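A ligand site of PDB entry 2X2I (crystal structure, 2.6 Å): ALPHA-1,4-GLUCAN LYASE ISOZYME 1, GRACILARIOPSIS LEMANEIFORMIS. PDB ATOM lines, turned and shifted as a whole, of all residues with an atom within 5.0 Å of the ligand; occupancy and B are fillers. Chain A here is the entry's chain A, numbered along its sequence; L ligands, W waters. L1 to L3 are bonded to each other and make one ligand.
CD1 of Leu 230 touches O3 of LG2 L2 (3.2 Å).
Phe 362 touches the ligand.
Val 402 touches the ligand.
O of Asp 501 touches C1 of LG3 L3, at 3.6 Å.
CE1 of Tyr 502 touches O7 of LG3 L3 (3.4 Å).
CZ2 of Trp 540 touches O5 of LG3 L3, 3.7 Å away.
OD2 of Asp 542 touches C9 of LG3 L3 (2.9 Å).
CZ2 of Trp 651 touches O5 of LG3 L3, 3.4 Å away.
CE1 of Phe 687 touches O6 of LG3 L3, at 3.6 Å.
CB of Thr 688 touches O6 of LIG L1 (3.95 Å).
His 720 touches the ligand.
Of the 26 residues printed, 19 come within 4 Å of the ligand.
Water W1 lies within hydrogen-bond range of an oxygen (O5) of LG3 L3 (2.8 Å), the indole nitrogen of Trp 651 (2.9 Å), a ring nitrogen (ND1) of His 720 (3.2 Å), the side-chain carboxylate of Asp 654 (3.4 Å) and the backbone carbonyl oxygen of Gly 653 (3.5 Å).
Water W2 lies within hydrogen-bond range of OH of Tyr 502 (2.8 Å), O7 of LG3 L3 (2.8 Å), ND2 of Asn 448 (2.9 Å) and OD2 of Asp 542 (2.9 Å).
OD2 of Asp 654 is in salt-bridge range of N1 of LG3 L3, at 2.9 Å.
A ring nitrogen (ND1) of His 730 lies close to an oxygen (O5) of LG2 L2 (3.2 Å).
The side-chain carboxylate (OD1) of Asp 228 lies within hydrogen-bond range of an oxygen (O1) of LG3 L3, 2.8 Å away.
An oxygen (O6) of LG3 L3 lies within hydrogen-bond range of the side-chain carboxylate (OD1) of Asp 401 (2.8 Å).
The guanidinium group (NH1) of Arg 638 is in hydrogen-bond range of an oxygen (O4) of LG3 L3, at 2.9 Å.
NE2 of Gln 234 is in hydrogen-bond range of O1 of LG2 L2 (3.0 Å).
The side-chain amide nitrogen (ND2) of Asn 448 sits at hydrogen-bond distance from an oxygen (O7) of LG3 L3 (2.9 Å).
The side-chain sulfur of Met 543 is in hydrogen-bond range of an oxygen (O2) of LG3 L3 (3.2 Å).
N of Asn 231 is in hydrogen-bond range of O of Asp 654 (2.9 Å).
The side-chain amide nitrogen (ND2) of Asn 448 lies within hydrogen-bond range of the side-chain carboxylate (OD2) of Asp 401, 2.9 Å away.
The side-chain carboxylate (OD1) of Asp 501 lies within hydrogen-bond range of the backbone NH (N) of Gly 503 (3.3 Å).
The guanidinium group (NH2) of Arg 638 sits close to the side-chain sulfur (SD) of Met 543 (3.7 Å).
NE2 of Gln 234 is in hydrogen-bond range of O of Leu 230 (3.2 Å).
ND1 of His 730 sits at hydrogen-bond distance from OD2 of Asp 722, 2.9 Å away.
The side-chain amide oxygen (OE1) of Gln 234 lies within hydrogen-bond range of the side-chain amino group (NZ) of Lys 579 (2.9 Å).
OD2 of Asp 654 is in salt-bridge range of NH1 of Arg 638 (3.8 Å).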
ATOM      1  N   ASP A 228     -12.364  16.866 -18.338  1.00  0.00           N
ATOM      2  CA  ASP A 228     -12.161  18.303 -18.341  1.00  0.00           C
ATOM      3  C   ASP A 228     -13.453  18.850 -17.700  1.00  0.00           C
ATOM      4  O   ASP A 228     -14.216  19.581 -18.314  1.00  0.00           O
ATOM      5  CB  ASP A 228     -11.969  18.750 -19.816  1.00  0.00           C
ATOM      6  CG  ASP A 228     -11.728  20.246 -19.976  1.00  0.00           C
ATOM      7  OD1 ASP A 228     -11.609  20.956 -18.959  1.00  0.00           O
ATOM      8  OD2 ASP A 228     -11.666  20.706 -21.134  1.00  0.00           O
ATOM      9  N   LEU A 230     -15.376  20.894 -15.850  1.00  0.00           N
ATOM     10  CA  LEU A 230     -15.521  22.195 -15.245  1.00  0.00           C
ATOM     11  C   LEU A 230     -16.862  22.287 -14.526  1.00  0.00           C
ATOM     12  O   LEU A 230     -17.912  22.047 -15.127  1.00  0.00           O
ATOM     13  CB  LEU A 230     -15.365  23.281 -16.323  1.00  0.00           C
ATOM     14  CG  LEU A 230     -15.756  24.715 -15.949  1.00  0.00           C
ATOM     15  CD1 LEU A 230     -14.791  25.711 -16.548  1.00  0.00           C
ATOM     16  CD2 LEU A 230     -17.202  25.033 -16.357  1.00  0.00           C
ATOM     17  N   ASN A 231     -16.810  22.610 -13.234  1.00  0.00           N
ATOM     18  CA  ASN A 231     -17.981  22.572 -12.314  1.00  0.00           C
ATOM     19  C   ASN A 231     -18.348  21.208 -11.782  1.00  0.00           C
ATOM     20  O   ASN A 231     -19.372  21.038 -11.158  1.00  0.00           O
ATOM     21  CB  ASN A 231     -19.194  23.240 -12.924  1.00  0.00           C
ATOM     22  CG  ASN A 231     -19.131  24.736 -12.825  1.00  0.00           C
ATOM     23  OD1 ASN A 231     -19.880  25.455 -13.461  1.00  0.00           O
ATOM     24  ND2 ASN A 231     -18.200  25.205 -12.030  1.00  0.00           N
ATOM     25  N   GLN A 234     -20.184  18.782 -15.858  1.00  0.00           N
ATOM     26  CA  GLN A 234     -20.242  18.978 -17.306  1.00  0.00           C
ATOM     27  C   GLN A 234     -21.416  18.271 -17.976  1.00  0.00           C
ATOM     28  O   GLN A 234     -21.673  17.080 -17.759  1.00  0.00           O
ATOM     29  CB  GLN A 234     -18.933  18.561 -17.973  1.00  0.00           C
ATOM     30  CG  GLN A 234     -17.930  19.685 -18.138  1.00  0.00           C
ATOM     31  CD  GLN A 234     -18.512  20.898 -18.859  1.00  0.00           C
ATOM     32  OE1 GLN A 234     -19.135  20.776 -19.918  1.00  0.00           O
ATOM     33  NE2 GLN A 234     -18.290  22.073 -18.303  1.00  0.00           N
ATOM     34  N   PHE A 362      -6.974  34.296 -13.571  1.00  0.00           N
ATOM     35  CA  PHE A 362      -7.094  34.099 -14.992  1.00  0.00           C
ATOM     36  C   PHE A 362      -7.614  35.356 -15.673  1.00  0.00           C
ATOM     37  O   PHE A 362      -8.815  35.490 -15.915  1.00  0.00           O
ATOM     38  CB  PHE A 362      -8.010  32.929 -15.297  1.00  0.00           C
ATOM     39  CG  PHE A 362      -8.051  32.593 -16.749  1.00  0.00           C
ATOM     40  CD1 PHE A 362      -6.980  32.920 -17.570  1.00  0.00           C
ATOM     41  CD2 PHE A 362      -9.144  31.947 -17.286  1.00  0.00           C
ATOM     42  CE1 PHE A 362      -7.002  32.618 -18.911  1.00  0.00           C
ATOM     43  CE2 PHE A 362      -9.171  31.634 -18.633  1.00  0.00           C
ATOM     44  CZ  PHE A 362      -8.091  31.963 -19.450  1.00  0.00           C
ATOM     45  N   ASP A 401      -0.972  32.897 -15.094  1.00  0.00           N
ATOM     46  CA  ASP A 401      -1.639  32.065 -16.086  1.00  0.00           C
ATOM     47  C   ASP A 401      -1.065  32.247 -17.506  1.00  0.00           C
ATOM     48  O   ASP A 401      -0.071  32.953 -17.745  1.00  0.00           O
ATOM     49  CB  ASP A 401      -3.147  32.342 -16.080  1.00  0.00           C
ATOM     50  CG  ASP A 401      -3.984  31.074 -16.174  1.00  0.00           C
ATOM     51  OD1 ASP A 401      -5.117  31.067 -15.658  1.00  0.00           O
ATOM     52  OD2 ASP A 401      -3.518  30.082 -16.767  1.00  0.00           O
ATOM     53  N   VAL A 402      -1.721  31.582 -18.456  1.00  0.00           N
ATOM     54  CA  VAL A 402      -1.381  31.661 -19.858  1.00  0.00           C
ATOM     55  C   VAL A 402      -1.474  33.092 -20.354  1.00  0.00           C
ATOM     56  O   VAL A 402      -1.000  33.394 -21.452  1.00  0.00           O
ATOM     57  CB  VAL A 402      -2.316  30.779 -20.690  1.00  0.00           C
ATOM     58  CG1 VAL A 402      -2.139  29.316 -20.309  1.00  0.00           C
ATOM     59  CG2 VAL A 402      -3.776  31.249 -20.516  1.00  0.00           C
ATOM     60  N   ASN A 448       1.402  28.503 -15.222  1.00  0.00           N
ATOM     61  CA  ASN A 448       0.661  27.446 -15.905  1.00  0.00           C
ATOM     62  C   ASN A 448       1.398  26.762 -17.074  1.00  0.00           C
ATOM     63  O   ASN A 448       1.769  27.439 -18.033  1.00  0.00           O
ATOM     64  CB  ASN A 448      -0.661  28.008 -16.403  1.00  0.00           C
ATOM     65  CG  ASN A 448      -1.589  26.932 -16.895  1.00  0.00           C
ATOM     66  OD1 ASN A 448      -1.270  25.755 -16.853  1.00  0.00           O
ATOM     67  ND2 ASN A 448      -2.750  27.339 -17.374  1.00  0.00           N
ATOM     68  N   ASP A 501      -9.545  25.317 -26.085  1.00  0.00           N
ATOM     69  CA  ASP A 501     -10.553  26.376 -25.952  1.00  0.00           C
ATOM     70  C   ASP A 501     -10.738  26.755 -24.495  1.00  0.00           C
ATOM     71  O   ASP A 501     -11.167  25.930 -23.680  1.00  0.00           O
ATOM     72  CB  ASP A 501     -11.894  25.946 -26.566  1.00  0.00           C
ATOM     73  CG  ASP A 501     -12.930  27.083 -26.575  1.00  0.00           C
ATOM     74  OD1 ASP A 501     -12.551  28.247 -26.823  1.00  0.00           O
ATOM     75  OD2 ASP A 501     -14.132  26.798 -26.356  1.00  0.00           O
ATOM     76  N   TYR A 502     -10.410  28.008 -24.176  1.00  0.00           N
ATOM     77  CA  TYR A 502     -10.562  28.545 -22.841  1.00  0.00           C
ATOM     78  C   TYR A 502     -11.730  29.503 -22.773  1.00  0.00           C
ATOM     79  O   TYR A 502     -11.824  30.268 -21.833  1.00  0.00           O
ATOM     80  CB  TYR A 502      -9.327  29.338 -22.410  1.00  0.00           C
ATOM     81  CG  TYR A 502      -8.049  28.550 -22.169  1.00  0.00           C
ATOM     82  CD1 TYR A 502      -7.971  27.561 -21.180  1.00  0.00           C
ATOM     83  CD2 TYR A 502      -6.904  28.847 -22.893  1.00  0.00           C
ATOM     84  CE1 TYR A 502      -6.773  26.871 -20.958  1.00  0.00           C
ATOM     85  CE2 TYR A 502      -5.730  28.171 -22.675  1.00  0.00           C
ATOM     86  CZ  TYR A 502      -5.654  27.186 -21.708  1.00  0.00           C
ATOM     87  OH  TYR A 502      -4.462  26.526 -21.535  1.00  0.00           O
ATOM     88  N   GLY A 503     -12.596  29.503 -23.782  1.00  0.00           N
ATOM     89  CA  GLY A 503     -13.768  30.385 -23.766  1.00  0.00           C
ATOM     90  C   GLY A 503     -13.508  31.738 -24.400  1.00  0.00           C
ATOM     91  O   GLY A 503     -12.349  32.141 -24.582  1.00  0.00           O
ATOM     92  N   TRP A 540       2.646  24.592 -12.470  1.00  0.00           N
ATOM     93  CA  TRP A 540       1.202  24.571 -12.388  1.00  0.00           C
ATOM     94  C   TRP A 540       0.755  23.734 -13.556  1.00  0.00           C
ATOM     95  O   TRP A 540       0.462  24.259 -14.615  1.00  0.00           O
ATOM     96  CB  TRP A 540       0.673  26.004 -12.488  1.00  0.00           C
ATOM     97  CG  TRP A 540      -0.825  26.194 -12.509  1.00  0.00           C
ATOM     98  CD1 TRP A 540      -1.785  25.260 -12.260  1.00  0.00           C
ATOM     99  CD2 TRP A 540      -1.526  27.442 -12.754  1.00  0.00           C
ATOM    100  NE1 TRP A 540      -3.051  25.835 -12.357  1.00  0.00           N
ATOM    101  CE2 TRP A 540      -2.913  27.166 -12.650  1.00  0.00           C
ATOM    102  CE3 TRP A 540      -1.115  28.732 -13.035  1.00  0.00           C
ATOM    103  CZ2 TRP A 540      -3.881  28.143 -12.849  1.00  0.00           C
ATOM    104  CZ3 TRP A 540      -2.089  29.715 -13.222  1.00  0.00           C
ATOM    105  CH2 TRP A 540      -3.451  29.406 -13.132  1.00  0.00           C
ATOM    106  N   ASP A 542      -1.554  21.957 -15.885  1.00  0.00           N
ATOM    107  CA  ASP A 542      -2.984  22.023 -16.207  1.00  0.00           C
ATOM    108  C   ASP A 542      -3.398  21.277 -17.488  1.00  0.00           C
ATOM    109  O   ASP A 542      -2.561  20.650 -18.156  1.00  0.00           O
ATOM    110  CB  ASP A 542      -3.397  23.489 -16.329  1.00  0.00           C
ATOM    111  CG  ASP A 542      -4.839  23.716 -16.009  1.00  0.00           C
ATOM    112  OD1 ASP A 542      -5.496  22.799 -15.453  1.00  0.00           O
ATOM    113  OD2 ASP A 542      -5.327  24.819 -16.302  1.00  0.00           O
ATOM    114  N   MET A 543      -4.685  21.364 -17.838  1.00  0.00           N
ATOM    115  CA  MET A 543      -5.319  20.665 -18.985  1.00  0.00           C
ATOM    116  C   MET A 543      -4.634  19.332 -19.286  1.00  0.00           C
ATOM    117  O   MET A 543      -4.282  19.036 -20.444  1.00  0.00           O
ATOM    118  CB  MET A 543      -5.362  21.560 -20.220  1.00  0.00           C
ATOM    119  CG  MET A 543      -5.920  22.960 -19.980  1.00  0.00           C
ATOM    120  SD  MET A 543      -7.700  23.098 -19.667  1.00  0.00           S
ATOM    121  CE  MET A 543      -8.398  23.163 -21.323  1.00  0.00           C
ATOM    122  N   LYS A 579     -13.598  15.289 -25.135  1.00  0.00           N
ATOM    123  CA  LYS A 579     -12.810  16.390 -24.622  1.00  0.00           C
ATOM    124  C   LYS A 579     -11.391  15.934 -24.308  1.00  0.00           C
ATOM    125  O   LYS A 579     -10.918  16.071 -23.200  1.00  0.00           O
ATOM    126  CB  LYS A 579     -13.510  17.010 -23.404  1.00  0.00           C
ATOM    127  CG  LYS A 579     -14.847  17.684 -23.755  1.00  0.00           C
ATOM    128  CD  LYS A 579     -15.349  18.538 -22.613  1.00  0.00           C
ATOM    129  CE  LYS A 579     -16.559  19.352 -23.011  1.00  0.00           C
ATOM    130  NZ  LYS A 579     -17.064  20.144 -21.836  1.00  0.00           N
ATOM    131  N   ARG A 638      -3.639  19.215 -12.025  1.00  0.00           N
ATOM    132  CA  ARG A 638      -5.095  19.095 -12.040  1.00  0.00           C
ATOM    133  C   ARG A 638      -5.585  17.671 -12.269  1.00  0.00           C
ATOM    134  O   ARG A 638      -6.668  17.287 -11.779  1.00  0.00           O
ATOM    135  CB  ARG A 638      -5.740  20.042 -13.051  1.00  0.00           C
ATOM    136  CG  ARG A 638      -7.174  20.450 -12.663  1.00  0.00           C
ATOM    137  CD  ARG A 638      -7.865  21.218 -13.757  1.00  0.00           C
ATOM    138  NE  ARG A 638      -7.860  20.488 -15.026  1.00  0.00           N
ATOM    139  CZ  ARG A 638      -8.309  21.011 -16.159  1.00  0.00           C
ATOM    140  NH1 ARG A 638      -8.795  22.235 -16.181  1.00  0.00           N
ATOM    141  NH2 ARG A 638      -8.274  20.301 -17.285  1.00  0.00           N
ATOM    142  N   TRP A 651      -4.688  20.382  -7.224  1.00  0.00           N
ATOM    143  CA  TRP A 651      -5.827  21.214  -6.896  1.00  0.00           C
ATOM    144  C   TRP A 651      -6.979  20.660  -7.684  1.00  0.00           C
ATOM    145  O   TRP A 651      -6.785  20.111  -8.769  1.00  0.00           O
ATOM    146  CB  TRP A 651      -5.568  22.673  -7.243  1.00  0.00           C
ATOM    147  CG  TRP A 651      -6.167  23.114  -8.521  1.00  0.00           C
ATOM    148  CD1 TRP A 651      -7.411  23.662  -8.699  1.00  0.00           C
ATOM    149  CD2 TRP A 651      -5.567  23.085  -9.826  1.00  0.00           C
ATOM    150  NE1 TRP A 651      -7.614  23.974 -10.015  1.00  0.00           N
ATOM    151  CE2 TRP A 651      -6.498  23.623 -10.734  1.00  0.00           C
ATOM    152  CE3 TRP A 651      -4.321  22.658 -10.306  1.00  0.00           C
ATOM    153  CZ2 TRP A 651      -6.223  23.759 -12.095  1.00  0.00           C
ATOM    154  CZ3 TRP A 651      -4.053  22.787 -11.650  1.00  0.00           C
ATOM    155  CH2 TRP A 651      -4.997  23.337 -12.536  1.00  0.00           C
ATOM    156  N   GLY A 653      -9.147  21.220  -9.898  1.00  0.00           N
ATOM    157  CA  GLY A 653      -9.643  21.864 -11.107  1.00  0.00           C
ATOM    158  C   GLY A 653     -10.667  22.939 -10.827  1.00  0.00           C
ATOM    159  O   GLY A 653     -10.516  23.745  -9.900  1.00  0.00           O
ATOM    160  N   ASP A 654     -11.739  22.908 -11.622  1.00  0.00           N
ATOM    161  CA  ASP A 654     -12.641  24.059 -11.732  1.00  0.00           C
ATOM    162  C   ASP A 654     -13.877  24.071 -10.887  1.00  0.00           C
ATOM    163  O   ASP A 654     -14.964  23.918 -11.404  1.00  0.00           O
ATOM    164  CB  ASP A 654     -13.053  24.267 -13.178  1.00  0.00           C
ATOM    165  CG  ASP A 654     -11.922  24.756 -14.009  1.00  0.00           C
ATOM    166  OD1 ASP A 654     -11.146  25.569 -13.479  1.00  0.00           O
ATOM    167  OD2 ASP A 654     -11.806  24.307 -15.167  1.00  0.00           O
ATOM    168  N   PHE A 687     -13.494  28.804  -8.659  1.00  0.00           N
ATOM    169  CA  PHE A 687     -12.944  29.265  -9.920  1.00  0.00           C
ATOM    170  C   PHE A 687     -13.960  29.961 -10.839  1.00  0.00           C
ATOM    171  O   PHE A 687     -13.746  31.085 -11.245  1.00  0.00           O
ATOM    172  CB  PHE A 687     -12.257  28.136 -10.680  1.00  0.00           C
ATOM    173  CG  PHE A 687     -11.748  28.561 -12.027  1.00  0.00           C
ATOM    174  CD1 PHE A 687     -10.624  29.323 -12.138  1.00  0.00           C
ATOM    175  CD2 PHE A 687     -12.425  28.214 -13.177  1.00  0.00           C
ATOM    176  CE1 PHE A 687     -10.166  29.725 -13.366  1.00  0.00           C
ATOM    177  CE2 PHE A 687     -11.989  28.609 -14.404  1.00  0.00           C
ATOM    178  CZ  PHE A 687     -10.853  29.364 -14.513  1.00  0.00           C
ATOM    179  N   THR A 688     -15.051  29.280 -11.173  1.00  0.00           N
ATOM    180  CA  THR A 688     -16.009  29.812 -12.139  1.00  0.00           C
ATOM    181  C   THR A 688     -17.021  30.774 -11.544  1.00  0.00           C
ATOM    182  O   THR A 688     -17.257  30.783 -10.331  1.00  0.00           O
ATOM    183  CB  THR A 688     -16.813  28.691 -12.825  1.00  0.00           C
ATOM    184  OG1 THR A 688     -17.560  27.982 -11.844  1.00  0.00           O
ATOM    185  CG2 THR A 688     -15.920  27.736 -13.577  1.00  0.00           C
ATOM    186  N   SER A 689     -17.640  31.582 -12.426  1.00  0.00           N
ATOM    187  CA  SER A 689     -18.778  32.451 -12.118  1.00  0.00           C
ATOM    188  C   SER A 689     -19.904  31.641 -11.481  1.00  0.00           C
ATOM    189  O   SER A 689     -19.909  30.426 -11.547  1.00  0.00           O
ATOM    190  CB  SER A 689     -19.300  33.095 -13.417  1.00  0.00           C
ATOM    191  OG  SER A 689     -18.316  33.848 -14.108  1.00  0.00           O
ATOM    192  N   ARG A 718      -4.902  28.356  -2.046  1.00  0.00           N
ATOM    193  CA  ARG A 718      -4.808  29.260  -3.169  1.00  0.00           C
ATOM    194  C   ARG A 718      -6.143  29.780  -3.642  1.00  0.00           C
ATOM    195  O   ARG A 718      -7.043  29.006  -4.002  1.00  0.00           O
ATOM    196  CB  ARG A 718      -4.094  28.628  -4.362  1.00  0.00           C
ATOM    197  CG  ARG A 718      -4.321  29.411  -5.608  1.00  0.00           C
ATOM    198  CD  ARG A 718      -3.704  28.758  -6.802  1.00  0.00           C
ATOM    199  NE  ARG A 718      -4.587  27.820  -7.453  1.00  0.00           N
ATOM    200  CZ  ARG A 718      -4.317  27.262  -8.624  1.00  0.00           C
ATOM    201  NH1 ARG A 718      -3.194  27.574  -9.260  1.00  0.00           N
ATOM    202  NH2 ARG A 718      -5.162  26.399  -9.176  1.00  0.00           N
ATOM    203  N   HIS A 720      -7.912  31.277  -6.494  1.00  0.00           N
ATOM    204  CA  HIS A 720      -7.802  31.420  -7.940  1.00  0.00           C
ATOM    205  C   HIS A 720      -9.173  31.542  -8.605  1.00  0.00           C
ATOM    206  O   HIS A 720     -10.145  30.951  -8.134  1.00  0.00           O
ATOM    207  CB  HIS A 720      -7.072  30.215  -8.541  1.00  0.00           C
ATOM    208  CG  HIS A 720      -6.918  30.296 -10.026  1.00  0.00           C
ATOM    209  ND1 HIS A 720      -7.397  29.319 -10.872  1.00  0.00           N
ATOM    210  CD2 HIS A 720      -6.325  31.221 -10.808  1.00  0.00           C
ATOM    211  CE1 HIS A 720      -7.106  29.638 -12.116  1.00  0.00           C
ATOM    212  NE2 HIS A 720      -6.449  30.791 -12.111  1.00  0.00           N
ATOM    213  N   ASP A 722     -11.545  32.729 -12.520  1.00  0.00           N
ATOM    214  CA  ASP A 722     -11.778  33.171 -13.880  1.00  0.00           C
ATOM    215  C   ASP A 722     -12.134  34.663 -13.800  1.00  0.00           C
ATOM    216  O   ASP A 722     -13.131  35.031 -13.175  1.00  0.00           O
ATOM    217  CB  ASP A 722     -12.958  32.325 -14.376  1.00  0.00           C
ATOM    218  CG  ASP A 722     -13.416  32.672 -15.791  1.00  0.00           C
ATOM    219  OD1 ASP A 722     -12.594  33.081 -16.623  1.00  0.00           O
ATOM    220  OD2 ASP A 722     -14.618  32.498 -16.053  1.00  0.00           O
ATOM    221  N   HIS A 730     -15.928  36.139 -20.163  1.00  0.00           N
ATOM    222  CA  HIS A 730     -16.502  35.267 -19.162  1.00  0.00           C
ATOM    223  C   HIS A 730     -15.710  35.336 -17.863  1.00  0.00           C
ATOM    224  O   HIS A 730     -14.466  35.411 -17.857  1.00  0.00           O
ATOM    225  CB  HIS A 730     -16.653  33.838 -19.679  1.00  0.00           C
ATOM    226  CG  HIS A 730     -15.357  33.136 -19.921  1.00  0.00           C
ATOM    227  ND1 HIS A 730     -14.619  32.573 -18.905  1.00  0.00           N
ATOM    228  CD2 HIS A 730     -14.681  32.878 -21.063  1.00  0.00           C
ATOM    229  CE1 HIS A 730     -13.536  32.011 -19.407  1.00  0.00           C
ATOM    230  NE2 HIS A 730     -13.552  32.190 -20.720  1.00  0.00           N
HETATM  231  C1  LIG L   1     -21.910  26.469 -18.425  1.00  0.00           C
HETATM  232  C2  LIG L   1     -20.595  25.954 -19.035  1.00  0.00           C
HETATM  233  C3  LIG L   1     -19.511  27.041 -19.068  1.00  0.00           C
HETATM  234  C4  LIG L   1     -19.448  27.742 -17.714  1.00  0.00           C
HETATM  235  C5  LIG L   1     -18.429  28.861 -17.602  1.00  0.00           C
HETATM  236  C6  LIG L   1     -21.568  27.138 -17.098  1.00  0.00           C
HETATM  237  O1  LIG L   1     -22.721  27.545 -16.351  1.00  0.00           O
HETATM  238  O2  LIG L   1     -22.816  25.385 -18.197  1.00  0.00           O
HETATM  239  O3  LIG L   1     -20.822  25.437 -20.341  1.00  0.00           O
HETATM  240  O4  LIG L   1     -18.217  26.458 -19.313  1.00  0.00           O
HETATM  241  O5  LIG L   1     -20.744  28.251 -17.428  1.00  0.00           O
HETATM  242  O6  LIG L   1     -18.548  29.457 -16.290  1.00  0.00           O
HETATM  243  C1  LG2 L   2     -17.844  26.411 -20.679  1.00  0.00           C
HETATM  244  C2  LG2 L   2     -17.252  25.036 -20.931  1.00  0.00           C
HETATM  245  C3  LG2 L   2     -15.960  24.819 -20.150  1.00  0.00           C
HETATM  246  C4  LG2 L   2     -14.974  25.958 -20.407  1.00  0.00           C
HETATM  247  C5  LG2 L   2     -15.685  27.296 -20.124  1.00  0.00           C
HETATM  248  C6  LG2 L   2     -14.796  28.516 -20.356  1.00  0.00           C
HETATM  249  O1  LG2 L   2     -18.222  24.098 -20.493  1.00  0.00           O
HETATM  250  O2  LG2 L   2     -15.328  23.596 -20.535  1.00  0.00           O
HETATM  251  O3  LG2 L   2     -13.776  25.740 -19.618  1.00  0.00           O
HETATM  252  O4  LG2 L   2     -16.871  27.405 -20.936  1.00  0.00           O
HETATM  253  O5  LG2 L   2     -15.458  29.669 -19.804  1.00  0.00           O
HETATM  254  C1  LG3 L   3     -12.524  25.729 -20.354  1.00  0.00           C
HETATM  255  O1  LG3 L   3     -12.311  23.276 -20.303  1.00  0.00           O
HETATM  256  C2  LG3 L   3     -11.666  24.514 -19.978  1.00  0.00           C
HETATM  257  C3  LG3 L   3      -6.935  27.804 -15.655  1.00  0.00           C
HETATM  258  C4  LG3 L   3     -11.354  24.522 -18.493  1.00  0.00           C
HETATM  259  O2  LG3 L   3     -10.480  23.436 -18.189  1.00  0.00           O
HETATM  260  C5  LG3 L   3     -10.641  25.833 -18.205  1.00  0.00           C
HETATM  261  N1  LG3 L   3     -10.072  25.852 -16.864  1.00  0.00           N
HETATM  262  C6  LG3 L   3     -11.543  26.997 -18.605  1.00  0.00           C
HETATM  263  O3  LG3 L   3     -11.757  26.884 -20.010  1.00  0.00           O
HETATM  264  C7  LG3 L   3     -10.926  28.355 -18.327  1.00  0.00           C
HETATM  265  C8  LG3 L   3      -8.630  25.660 -16.866  1.00  0.00           C
HETATM  266  C9  LG3 L   3      -8.028  25.557 -15.466  1.00  0.00           C
HETATM  267  O4  LG3 L   3      -8.778  24.665 -14.631  1.00  0.00           O
HETATM  268  C10 LG3 L   3      -7.848  26.909 -14.806  1.00  0.00           C
HETATM  269  O5  LG3 L   3      -7.135  26.630 -13.607  1.00  0.00           O
HETATM  270  O6  LG3 L   3      -7.126  29.160 -15.264  1.00  0.00           O
HETATM  271  C11 LG3 L   3      -7.194  27.711 -17.116  1.00  0.00           C
HETATM  272  C12 LG3 L   3      -7.956  26.754 -17.658  1.00  0.00           C
HETATM  273  C13 LG3 L   3      -6.572  28.741 -18.031  1.00  0.00           C
HETATM  274  O7  LG3 L   3      -5.246  28.337 -18.358  1.00  0.00           O
HETATM  275  O   HOH W   1      -8.685  26.375 -11.305  1.00  0.00           O
HETATM  276  O   HOH W   2      -4.498  25.672 -18.910  1.00  0.00           O
